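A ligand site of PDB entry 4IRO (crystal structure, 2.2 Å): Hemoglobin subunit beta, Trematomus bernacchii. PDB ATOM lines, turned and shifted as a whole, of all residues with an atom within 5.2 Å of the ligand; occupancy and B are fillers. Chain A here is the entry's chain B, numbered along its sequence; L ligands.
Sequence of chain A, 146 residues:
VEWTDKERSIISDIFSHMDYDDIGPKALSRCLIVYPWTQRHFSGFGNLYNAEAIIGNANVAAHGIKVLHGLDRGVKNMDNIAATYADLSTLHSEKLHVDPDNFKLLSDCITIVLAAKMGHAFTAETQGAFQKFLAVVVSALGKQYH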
ATOM      1  N   LEU A  32      29.381  35.037 -23.507  1.00  0.00           N
ATOM      2  CA  LEU A  32      29.173  35.916 -22.364  1.00  0.00           C
ATOM      3  C   LEU A  32      29.385  37.376 -22.770  1.00  0.00           C
ATOM      4  O   LEU A  32      28.827  38.270 -22.151  1.00  0.00           O
ATOM      5  CB  LEU A  32      30.111  35.521 -21.224  1.00  0.00           C
ATOM      6  CG  LEU A  32      29.627  34.403 -20.306  1.00  0.00           C
ATOM      7  CD1 LEU A  32      29.602  34.869 -18.858  1.00  0.00           C
ATOM      8  CD2 LEU A  32      28.253  33.880 -20.711  1.00  0.00           C
ATOM      9  N   THR A  38      23.808  36.996 -20.709  1.00  0.00           N
ATOM     10  CA  THR A  38      24.080  35.614 -20.327  1.00  0.00           C
ATOM     11  C   THR A  38      25.217  35.514 -19.309  1.00  0.00           C
ATOM     12  O   THR A  38      25.647  34.407 -18.985  1.00  0.00           O
ATOM     13  CB  THR A  38      24.422  34.749 -21.550  1.00  0.00           C
ATOM     14  OG1 THR A  38      25.785  34.957 -21.930  1.00  0.00           O
ATOM     15  CG2 THR A  38      23.557  35.143 -22.732  1.00  0.00           C
ATOM     16  N   HIS A  41      23.673  34.557 -15.137  1.00  0.00           N
ATOM     17  CA  HIS A  41      23.689  33.271 -14.464  1.00  0.00           C
ATOM     18  C   HIS A  41      25.113  32.848 -14.118  1.00  0.00           C
ATOM     19  O   HIS A  41      25.398  31.678 -13.887  1.00  0.00           O
ATOM     20  CB  HIS A  41      23.022  32.235 -15.367  1.00  0.00           C
ATOM     21  CG  HIS A  41      21.910  32.748 -16.220  1.00  0.00           C
ATOM     22  ND1 HIS A  41      20.580  32.452 -15.983  1.00  0.00           N
ATOM     23  CD2 HIS A  41      21.902  33.529 -17.327  1.00  0.00           C
ATOM     24  CE1 HIS A  41      19.825  33.038 -16.896  1.00  0.00           C
ATOM     25  NE2 HIS A  41      20.595  33.701 -17.725  1.00  0.00           N
ATOM     26  N   PHE A  42      26.042  33.803 -14.069  1.00  0.00           N
ATOM     27  CA  PHE A  42      27.427  33.495 -13.712  1.00  0.00           C
ATOM     28  C   PHE A  42      27.957  34.525 -12.719  1.00  0.00           C
ATOM     29  O   PHE A  42      29.071  35.017 -12.822  1.00  0.00           O
ATOM     30  CB  PHE A  42      28.286  33.402 -14.986  1.00  0.00           C
ATOM     31  CG  PHE A  42      27.846  32.218 -15.848  1.00  0.00           C
ATOM     32  CD1 PHE A  42      28.165  30.919 -15.470  1.00  0.00           C
ATOM     33  CD2 PHE A  42      27.131  32.403 -17.008  1.00  0.00           C
ATOM     34  CE1 PHE A  42      27.774  29.835 -16.212  1.00  0.00           C
ATOM     35  CE2 PHE A  42      26.743  31.324 -17.772  1.00  0.00           C
ATOM     36  CZ  PHE A  42      27.038  30.032 -17.376  1.00  0.00           C
ATOM     37  N   HIS A  63      31.808  24.940 -16.881  1.00  0.00           N
ATOM     38  CA  HIS A  63      30.499  24.849 -17.515  1.00  0.00           C
ATOM     39  C   HIS A  63      30.651  24.711 -19.024  1.00  0.00           C
ATOM     40  O   HIS A  63      29.869  24.023 -19.678  1.00  0.00           O
ATOM     41  CB  HIS A  63      29.647  26.068 -17.148  1.00  0.00           C
ATOM     42  CG  HIS A  63      28.260  26.027 -17.709  1.00  0.00           C
ATOM     43  ND1 HIS A  63      27.868  26.699 -18.841  1.00  0.00           N
ATOM     44  CD2 HIS A  63      27.153  25.369 -17.294  1.00  0.00           C
ATOM     45  CE1 HIS A  63      26.596  26.469 -19.090  1.00  0.00           C
ATOM     46  NE2 HIS A  63      26.131  25.657 -18.159  1.00  0.00           N
ATOM     47  N   LYS A  66      31.532  21.233 -19.285  1.00  0.00           N
ATOM     48  CA  LYS A  66      30.298  20.686 -18.762  1.00  0.00           C
ATOM     49  C   LYS A  66      29.274  20.496 -19.882  1.00  0.00           C
ATOM     50  O   LYS A  66      28.641  19.432 -19.984  1.00  0.00           O
ATOM     51  CB  LYS A  66      29.677  21.599 -17.709  1.00  0.00           C
ATOM     52  CG  LYS A  66      29.893  21.210 -16.259  1.00  0.00           C
ATOM     53  CD  LYS A  66      29.974  22.424 -15.347  1.00  0.00           C
ATOM     54  CE  LYS A  66      28.667  23.209 -15.314  1.00  0.00           C
ATOM     55  NZ  LYS A  66      28.531  24.006 -14.045  1.00  0.00           N
ATOM     56  N   VAL A  67      29.124  21.526 -20.702  1.00  0.00           N
ATOM     57  CA  VAL A  67      28.074  21.634 -21.693  1.00  0.00           C
ATOM     58  C   VAL A  67      28.329  20.716 -22.870  1.00  0.00           C
ATOM     59  O   VAL A  67      27.428  20.131 -23.481  1.00  0.00           O
ATOM     60  CB  VAL A  67      27.922  23.088 -22.214  1.00  0.00           C
ATOM     61  CG1 VAL A  67      27.009  23.130 -23.430  1.00  0.00           C
ATOM     62  CG2 VAL A  67      27.396  24.013 -21.136  1.00  0.00           C
ATOM     63  N   GLY A  70      27.433  17.196 -21.927  1.00  0.00           N
ATOM     64  CA  GLY A  70      26.000  17.017 -21.850  1.00  0.00           C
ATOM     65  C   GLY A  70      25.351  16.771 -23.181  1.00  0.00           C
ATOM     66  O   GLY A  70      24.203  16.331 -23.255  1.00  0.00           O
ATOM     67  N   LEU A  71      26.037  17.042 -24.294  1.00  0.00           N
ATOM     68  CA  LEU A  71      25.391  16.733 -25.573  1.00  0.00           C
ATOM     69  C   LEU A  71      25.753  15.321 -26.007  1.00  0.00           C
ATOM     70  O   LEU A  71      25.100  14.733 -26.876  1.00  0.00           O
ATOM     71  CB  LEU A  71      25.781  17.754 -26.640  1.00  0.00           C
ATOM     72  CG  LEU A  71      25.490  19.218 -26.310  1.00  0.00           C
ATOM     73  CD1 LEU A  71      26.784  20.004 -26.198  1.00  0.00           C
ATOM     74  CD2 LEU A  71      24.554  19.828 -27.349  1.00  0.00           C
ATOM     75  N   ARG A  73      25.232  12.794 -24.390  1.00  0.00           N
ATOM     76  CA  ARG A  73      24.023  12.029 -24.090  1.00  0.00           C
ATOM     77  C   ARG A  73      23.049  12.101 -25.259  1.00  0.00           C
ATOM     78  O   ARG A  73      22.359  11.143 -25.594  1.00  0.00           O
ATOM     79  CB  ARG A  73      23.369  12.515 -22.806  1.00  0.00           C
ATOM     80  CG  ARG A  73      22.803  13.920 -22.845  1.00  0.00           C
ATOM     81  CD  ARG A  73      22.772  14.516 -21.448  1.00  0.00           C
ATOM     82  NE  ARG A  73      24.101  14.496 -20.839  1.00  0.00           N
ATOM     83  CZ  ARG A  73      24.415  15.020 -19.664  1.00  0.00           C
ATOM     84  NH1 ARG A  73      23.474  15.603 -18.933  1.00  0.00           N
ATOM     85  NH2 ARG A  73      25.657  14.952 -19.206  1.00  0.00           N
ATOM     86  N   TYR A  85      17.031  15.155 -21.709  1.00  0.00           N
ATOM     87  CA  TYR A  85      17.511  16.345 -20.984  1.00  0.00           C
ATOM     88  C   TYR A  85      16.537  16.792 -19.899  1.00  0.00           C
ATOM     89  O   TYR A  85      16.748  17.846 -19.303  1.00  0.00           O
ATOM     90  CB  TYR A  85      17.794  17.474 -22.000  1.00  0.00           C
ATOM     91  CG  TYR A  85      19.057  17.159 -22.773  1.00  0.00           C
ATOM     92  CD1 TYR A  85      20.294  17.440 -22.213  1.00  0.00           C
ATOM     93  CD2 TYR A  85      19.004  16.591 -24.032  1.00  0.00           C
ATOM     94  CE1 TYR A  85      21.453  17.161 -22.905  1.00  0.00           C
ATOM     95  CE2 TYR A  85      20.165  16.303 -24.735  1.00  0.00           C
ATOM     96  CZ  TYR A  85      21.379  16.592 -24.158  1.00  0.00           C
ATOM     97  OH  TYR A  85      22.541  16.313 -24.840  1.00  0.00           O
ATOM     98  N   LEU A  88      17.738  18.014 -16.706  1.00  0.00           N
ATOM     99  CA  LEU A  88      18.634  19.142 -16.961  1.00  0.00           C
ATOM    100  C   LEU A  88      17.838  20.436 -17.152  1.00  0.00           C
ATOM    101  O   LEU A  88      18.254  21.503 -16.687  1.00  0.00           O
ATOM    102  CB  LEU A  88      19.518  18.849 -18.178  1.00  0.00           C
ATOM    103  CG  LEU A  88      21.009  19.137 -18.002  1.00  0.00           C
ATOM    104  CD1 LEU A  88      21.390  19.175 -16.531  1.00  0.00           C
ATOM    105  CD2 LEU A  88      21.855  18.107 -18.754  1.00  0.00           C
ATOM    106  N   LEU A  91      16.393  21.548 -13.838  1.00  0.00           N
ATOM    107  CA  LEU A  91      17.542  22.151 -13.152  1.00  0.00           C
ATOM    108  C   LEU A  91      17.652  23.620 -13.519  1.00  0.00           C
ATOM    109  O   LEU A  91      17.460  24.506 -12.682  1.00  0.00           O
ATOM    110  CB  LEU A  91      18.818  21.397 -13.519  1.00  0.00           C
ATOM    111  CG  LEU A  91      20.132  21.896 -12.921  1.00  0.00           C
ATOM    112  CD1 LEU A  91      20.103  21.802 -11.404  1.00  0.00           C
ATOM    113  CD2 LEU A  91      21.320  21.135 -13.482  1.00  0.00           C
ATOM    114  N   HIS A  92      17.952  23.868 -14.782  1.00  0.00           N
ATOM    115  CA  HIS A  92      18.194  25.221 -15.290  1.00  0.00           C
ATOM    116  C   HIS A  92      16.956  26.080 -15.038  1.00  0.00           C
ATOM    117  O   HIS A  92      17.045  27.273 -14.752  1.00  0.00           O
ATOM    118  CB  HIS A  92      18.565  25.195 -16.768  1.00  0.00           C
ATOM    119  CG  HIS A  92      19.955  24.732 -17.066  1.00  0.00           C
ATOM    120  ND1 HIS A  92      20.329  23.404 -17.088  1.00  0.00           N
ATOM    121  CD2 HIS A  92      21.087  25.431 -17.354  1.00  0.00           C
ATOM    122  CE1 HIS A  92      21.609  23.304 -17.379  1.00  0.00           C
ATOM    123  NE2 HIS A  92      22.100  24.523 -17.541  1.00  0.00           N
ATOM    124  N   LEU A  96      18.378  27.180 -11.533  1.00  0.00           N
ATOM    125  CA  LEU A  96      19.349  27.982 -12.254  1.00  0.00           C
ATOM    126  C   LEU A  96      18.720  29.238 -12.845  1.00  0.00           C
ATOM    127  O   LEU A  96      19.424  30.189 -13.210  1.00  0.00           O
ATOM    128  CB  LEU A  96      19.991  27.133 -13.355  1.00  0.00           C
ATOM    129  CG  LEU A  96      20.878  25.981 -12.859  1.00  0.00           C
ATOM    130  CD1 LEU A  96      21.547  25.281 -14.021  1.00  0.00           C
ATOM    131  CD2 LEU A  96      21.899  26.507 -11.865  1.00  0.00           C
ATOM    132  N   VAL A  98      17.695  29.817 -15.605  1.00  0.00           N
ATOM    133  CA  VAL A  98      18.286  30.121 -16.899  1.00  0.00           C
ATOM    134  C   VAL A  98      17.231  30.515 -17.912  1.00  0.00           C
ATOM    135  O   VAL A  98      16.299  29.776 -18.201  1.00  0.00           O
ATOM    136  CB  VAL A  98      19.069  28.931 -17.486  1.00  0.00           C
ATOM    137  CG1 VAL A  98      19.278  29.163 -18.972  1.00  0.00           C
ATOM    138  CG2 VAL A  98      20.394  28.723 -16.770  1.00  0.00           C
ATOM    139  N   ASN A 102      18.521  31.932 -23.773  1.00  0.00           N
ATOM    140  CA  ASN A 102      19.947  31.747 -23.564  1.00  0.00           C
ATOM    141  C   ASN A 102      20.489  30.530 -24.301  1.00  0.00           C
ATOM    142  O   ASN A 102      21.678  30.466 -24.629  1.00  0.00           O
ATOM    143  CB  ASN A 102      20.244  31.634 -22.067  1.00  0.00           C
ATOM    144  CG  ASN A 102      20.207  32.960 -21.341  1.00  0.00           C
ATOM    145  OD1 ASN A 102      20.291  33.023 -20.107  1.00  0.00           O
ATOM    146  ND2 ASN A 102      20.089  34.054 -22.087  1.00  0.00           N
ATOM    147  N   PHE A 103      19.640  29.548 -24.580  1.00  0.00           N
ATOM    148  CA  PHE A 103      20.043  28.268 -25.141  1.00  0.00           C
ATOM    149  C   PHE A 103      20.470  28.404 -26.595  1.00  0.00           C
ATOM    150  O   PHE A 103      21.535  27.906 -26.977  1.00  0.00           O
ATOM    151  CB  PHE A 103      18.913  27.237 -25.007  1.00  0.00           C
ATOM    152  CG  PHE A 103      18.590  26.948 -23.540  1.00  0.00           C
ATOM    153  CD1 PHE A 103      19.600  26.637 -22.639  1.00  0.00           C
ATOM    154  CD2 PHE A 103      17.291  27.003 -23.076  1.00  0.00           C
ATOM    155  CE1 PHE A 103      19.314  26.399 -21.308  1.00  0.00           C
ATOM    156  CE2 PHE A 103      17.001  26.773 -21.744  1.00  0.00           C
ATOM    157  CZ  PHE A 103      18.017  26.467 -20.855  1.00  0.00           C
ATOM    158  N   LEU A 106      23.971  30.331 -26.986  1.00  0.00           N
ATOM    159  CA  LEU A 106      25.051  29.371 -26.797  1.00  0.00           C
ATOM    160  C   LEU A 106      25.144  28.375 -27.948  1.00  0.00           C
ATOM    161  O   LEU A 106      26.225  27.971 -28.377  1.00  0.00           O
ATOM    162  CB  LEU A 106      24.840  28.625 -25.472  1.00  0.00           C
ATOM    163  CG  LEU A 106      26.034  27.830 -24.973  1.00  0.00           C
ATOM    164  CD1 LEU A 106      27.326  28.607 -25.213  1.00  0.00           C
ATOM    165  CD2 LEU A 106      25.902  27.481 -23.497  1.00  0.00           C
ATOM    166  N   ILE A 110      28.525  27.928 -30.156  1.00  0.00           N
ATOM    167  CA  ILE A 110      29.263  26.665 -30.230  1.00  0.00           C
ATOM    168  C   ILE A 110      29.634  26.441 -31.685  1.00  0.00           C
ATOM    169  O   ILE A 110      30.723  26.006 -32.023  1.00  0.00           O
ATOM    170  CB  ILE A 110      28.465  25.468 -29.690  1.00  0.00           C
ATOM    171  CG1 ILE A 110      28.589  25.272 -28.174  1.00  0.00           C
ATOM    172  CG2 ILE A 110      28.856  24.178 -30.393  1.00  0.00           C
ATOM    173  CD1 ILE A 110      27.272  25.120 -27.444  1.00  0.00           C
ATOM    174  N   LEU A 141      15.838  21.504 -23.860  1.00  0.00           N
ATOM    175  CA  LEU A 141      16.473  22.158 -22.716  1.00  0.00           C
ATOM    176  C   LEU A 141      15.613  23.259 -22.117  1.00  0.00           C
ATOM    177  O   LEU A 141      15.575  23.465 -20.901  1.00  0.00           O
ATOM    178  CB  LEU A 141      17.847  22.697 -23.144  1.00  0.00           C
ATOM    179  CG  LEU A 141      19.044  21.822 -22.791  1.00  0.00           C
ATOM    180  CD1 LEU A 141      20.348  22.528 -23.127  1.00  0.00           C
ATOM    181  CD2 LEU A 141      19.010  21.423 -21.322  1.00  0.00           C
HETATM  182  C1  LIG L   1      25.466  24.208 -14.712  1.00  0.00           C
HETATM  183  C2  LIG L   1      24.408  22.040 -18.904  1.00  0.00           C
HETATM  184  C3  LIG L   1      23.445  26.348 -20.852  1.00  0.00           C
HETATM  185  C4  LIG L   1      23.852  28.386 -16.495  1.00  0.00           C
HETATM  186  C5  LIG L   1      25.215  23.215 -15.651  1.00  0.00           C
HETATM  187  C6  LIG L   1      25.191  21.799 -15.413  1.00  0.00           C
HETATM  188  C7  LIG L   1      24.896  21.204 -16.582  1.00  0.00           C
HETATM  189  C8  LIG L   1      24.724  22.247 -17.572  1.00  0.00           C
HETATM  190  C9  LIG L   1      24.723  19.707 -16.893  1.00  0.00           C
HETATM  191  C10 LIG L   1      25.500  21.110 -14.070  1.00  0.00           C
HETATM  192  C11 LIG L   1      24.871  21.610 -12.793  1.00  0.00           C
HETATM  193  C12 LIG L   1      25.772  22.454 -11.914  1.00  0.00           C
HETATM  194  O1  LIG L   1      26.875  22.804 -12.419  1.00  0.00           O
HETATM  195  O2  LIG L   1      25.344  22.748 -10.765  1.00  0.00           O
HETATM  196  C13 LIG L   1      24.108  23.015 -19.816  1.00  0.00           C
HETATM  197  C14 LIG L   1      23.857  22.820 -21.229  1.00  0.00           C
HETATM  198  C15 LIG L   1      23.633  24.012 -21.779  1.00  0.00           C
HETATM  199  C16 LIG L   1      23.688  24.997 -20.712  1.00  0.00           C
HETATM  200  C17 LIG L   1      23.878  21.422 -21.909  1.00  0.00           C
HETATM  201  C18 LIG L   1      23.279  24.373 -23.231  1.00  0.00           C
HETATM  202  C19 LIG L   1      23.879  23.741 -24.249  1.00  0.00           C
HETATM  203  C20 LIG L   1      23.477  27.282 -19.840  1.00  0.00           C
HETATM  204  C21 LIG L   1      23.289  28.703 -20.018  1.00  0.00           C
HETATM  205  C22 LIG L   1      23.387  29.268 -18.814  1.00  0.00           C
HETATM  206  C23 LIG L   1      23.640  28.215 -17.847  1.00  0.00           C
HETATM  207  C24 LIG L   1      23.018  29.358 -21.382  1.00  0.00           C
HETATM  208  C25 LIG L   1      23.327  30.768 -18.436  1.00  0.00           C
HETATM  209  C26 LIG L   1      23.890  31.692 -19.218  1.00  0.00           C
HETATM  210  C27 LIG L   1      24.338  27.437 -15.626  1.00  0.00           C
HETATM  211  C28 LIG L   1      24.658  27.647 -14.232  1.00  0.00           C
HETATM  212  C29 LIG L   1      25.115  26.496 -13.739  1.00  0.00           C
HETATM  213  C30 LIG L   1      25.020  25.510 -14.784  1.00  0.00           C
HETATM  214  C31 LIG L   1      24.495  29.013 -13.533  1.00  0.00           C
HETATM  215  C32 LIG L   1      25.534  26.170 -12.285  1.00  0.00           C
HETATM  216  C33 LIG L   1      26.956  25.689 -12.020  1.00  0.00           C
HETATM  217  C34 LIG L   1      27.322  25.472 -10.573  1.00  0.00           C
HETATM  218  O3  LIG L   1      28.339  24.769 -10.337  1.00  0.00           O
HETATM  219  O4  LIG L   1      26.578  26.004  -9.711  1.00  0.00           O
HETATM  220  N1  LIG L   1      24.926  23.480 -16.985  1.00  0.00           N
HETATM  221  N2  LIG L   1      23.991  24.370 -19.513  1.00  0.00           N
HETATM  222  N3  LIG L   1      23.701  27.006 -18.508  1.00  0.00           N
HETATM  223  N4  LIG L   1      24.595  26.114 -15.958  1.00  0.00           N
HETATM  224 FE1  LIG L   1      24.146  25.209 -17.693  1.00  0.00          FE
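FE1 of the ligand is bound by NE2 of His 63, 2.1 Å away. A ring nitrogen (NE2) of His 92 is bound to an iron atom (FE1) of the ligand (2.2 Å). The side-chain amino group of Lys 66 is in salt-bridge range of an oxygen (O1) of the ligand (2.6 Å).
The backbone carbonyl oxygen of Leu 88 sits at hydrogen-bond distance from a ring nitrogen (ND1) of His 92. The side-chain amide oxygen (OD1) of Asn 102 sits at hydrogen-bond distance from a ring nitrogen (NE2) of His 41, at 2.5 Å. N of Val 98 sits at hydrogen-bond distance from O of His 92, at 2.8 Å. The backbone NH (N) of Leu 96 lies within hydrogen-bond range of the backbone carbonyl oxygen (O) of Leu 91.
Thr 38 touches the ligand. O of His 41 touches C31 of the ligand, 2.8 Å away. CE2 of Phe 42 touches C26 of the ligand (3.2 Å). Val 67 touches the ligand. Leu 88 touches the ligand. CD2 of Leu 91 touches C11 of the ligand, 3.6 Å away. Leu 96 touches the ligand (CD1 to C30, 3.6 Å). CG2 of Val 98 touches C23 of the ligand, at 3.5 Å. CB of Asn 102 touches C24 of the ligand, 3.7 Å away. Leu 106 touches the ligand (CD2 to C3, 3.8 Å). CD1 of Leu 141 touches C18 of the ligand (3.5 Å). The nearest printed residue that does not touch the ligand is Phe 103 (4.2 Å).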
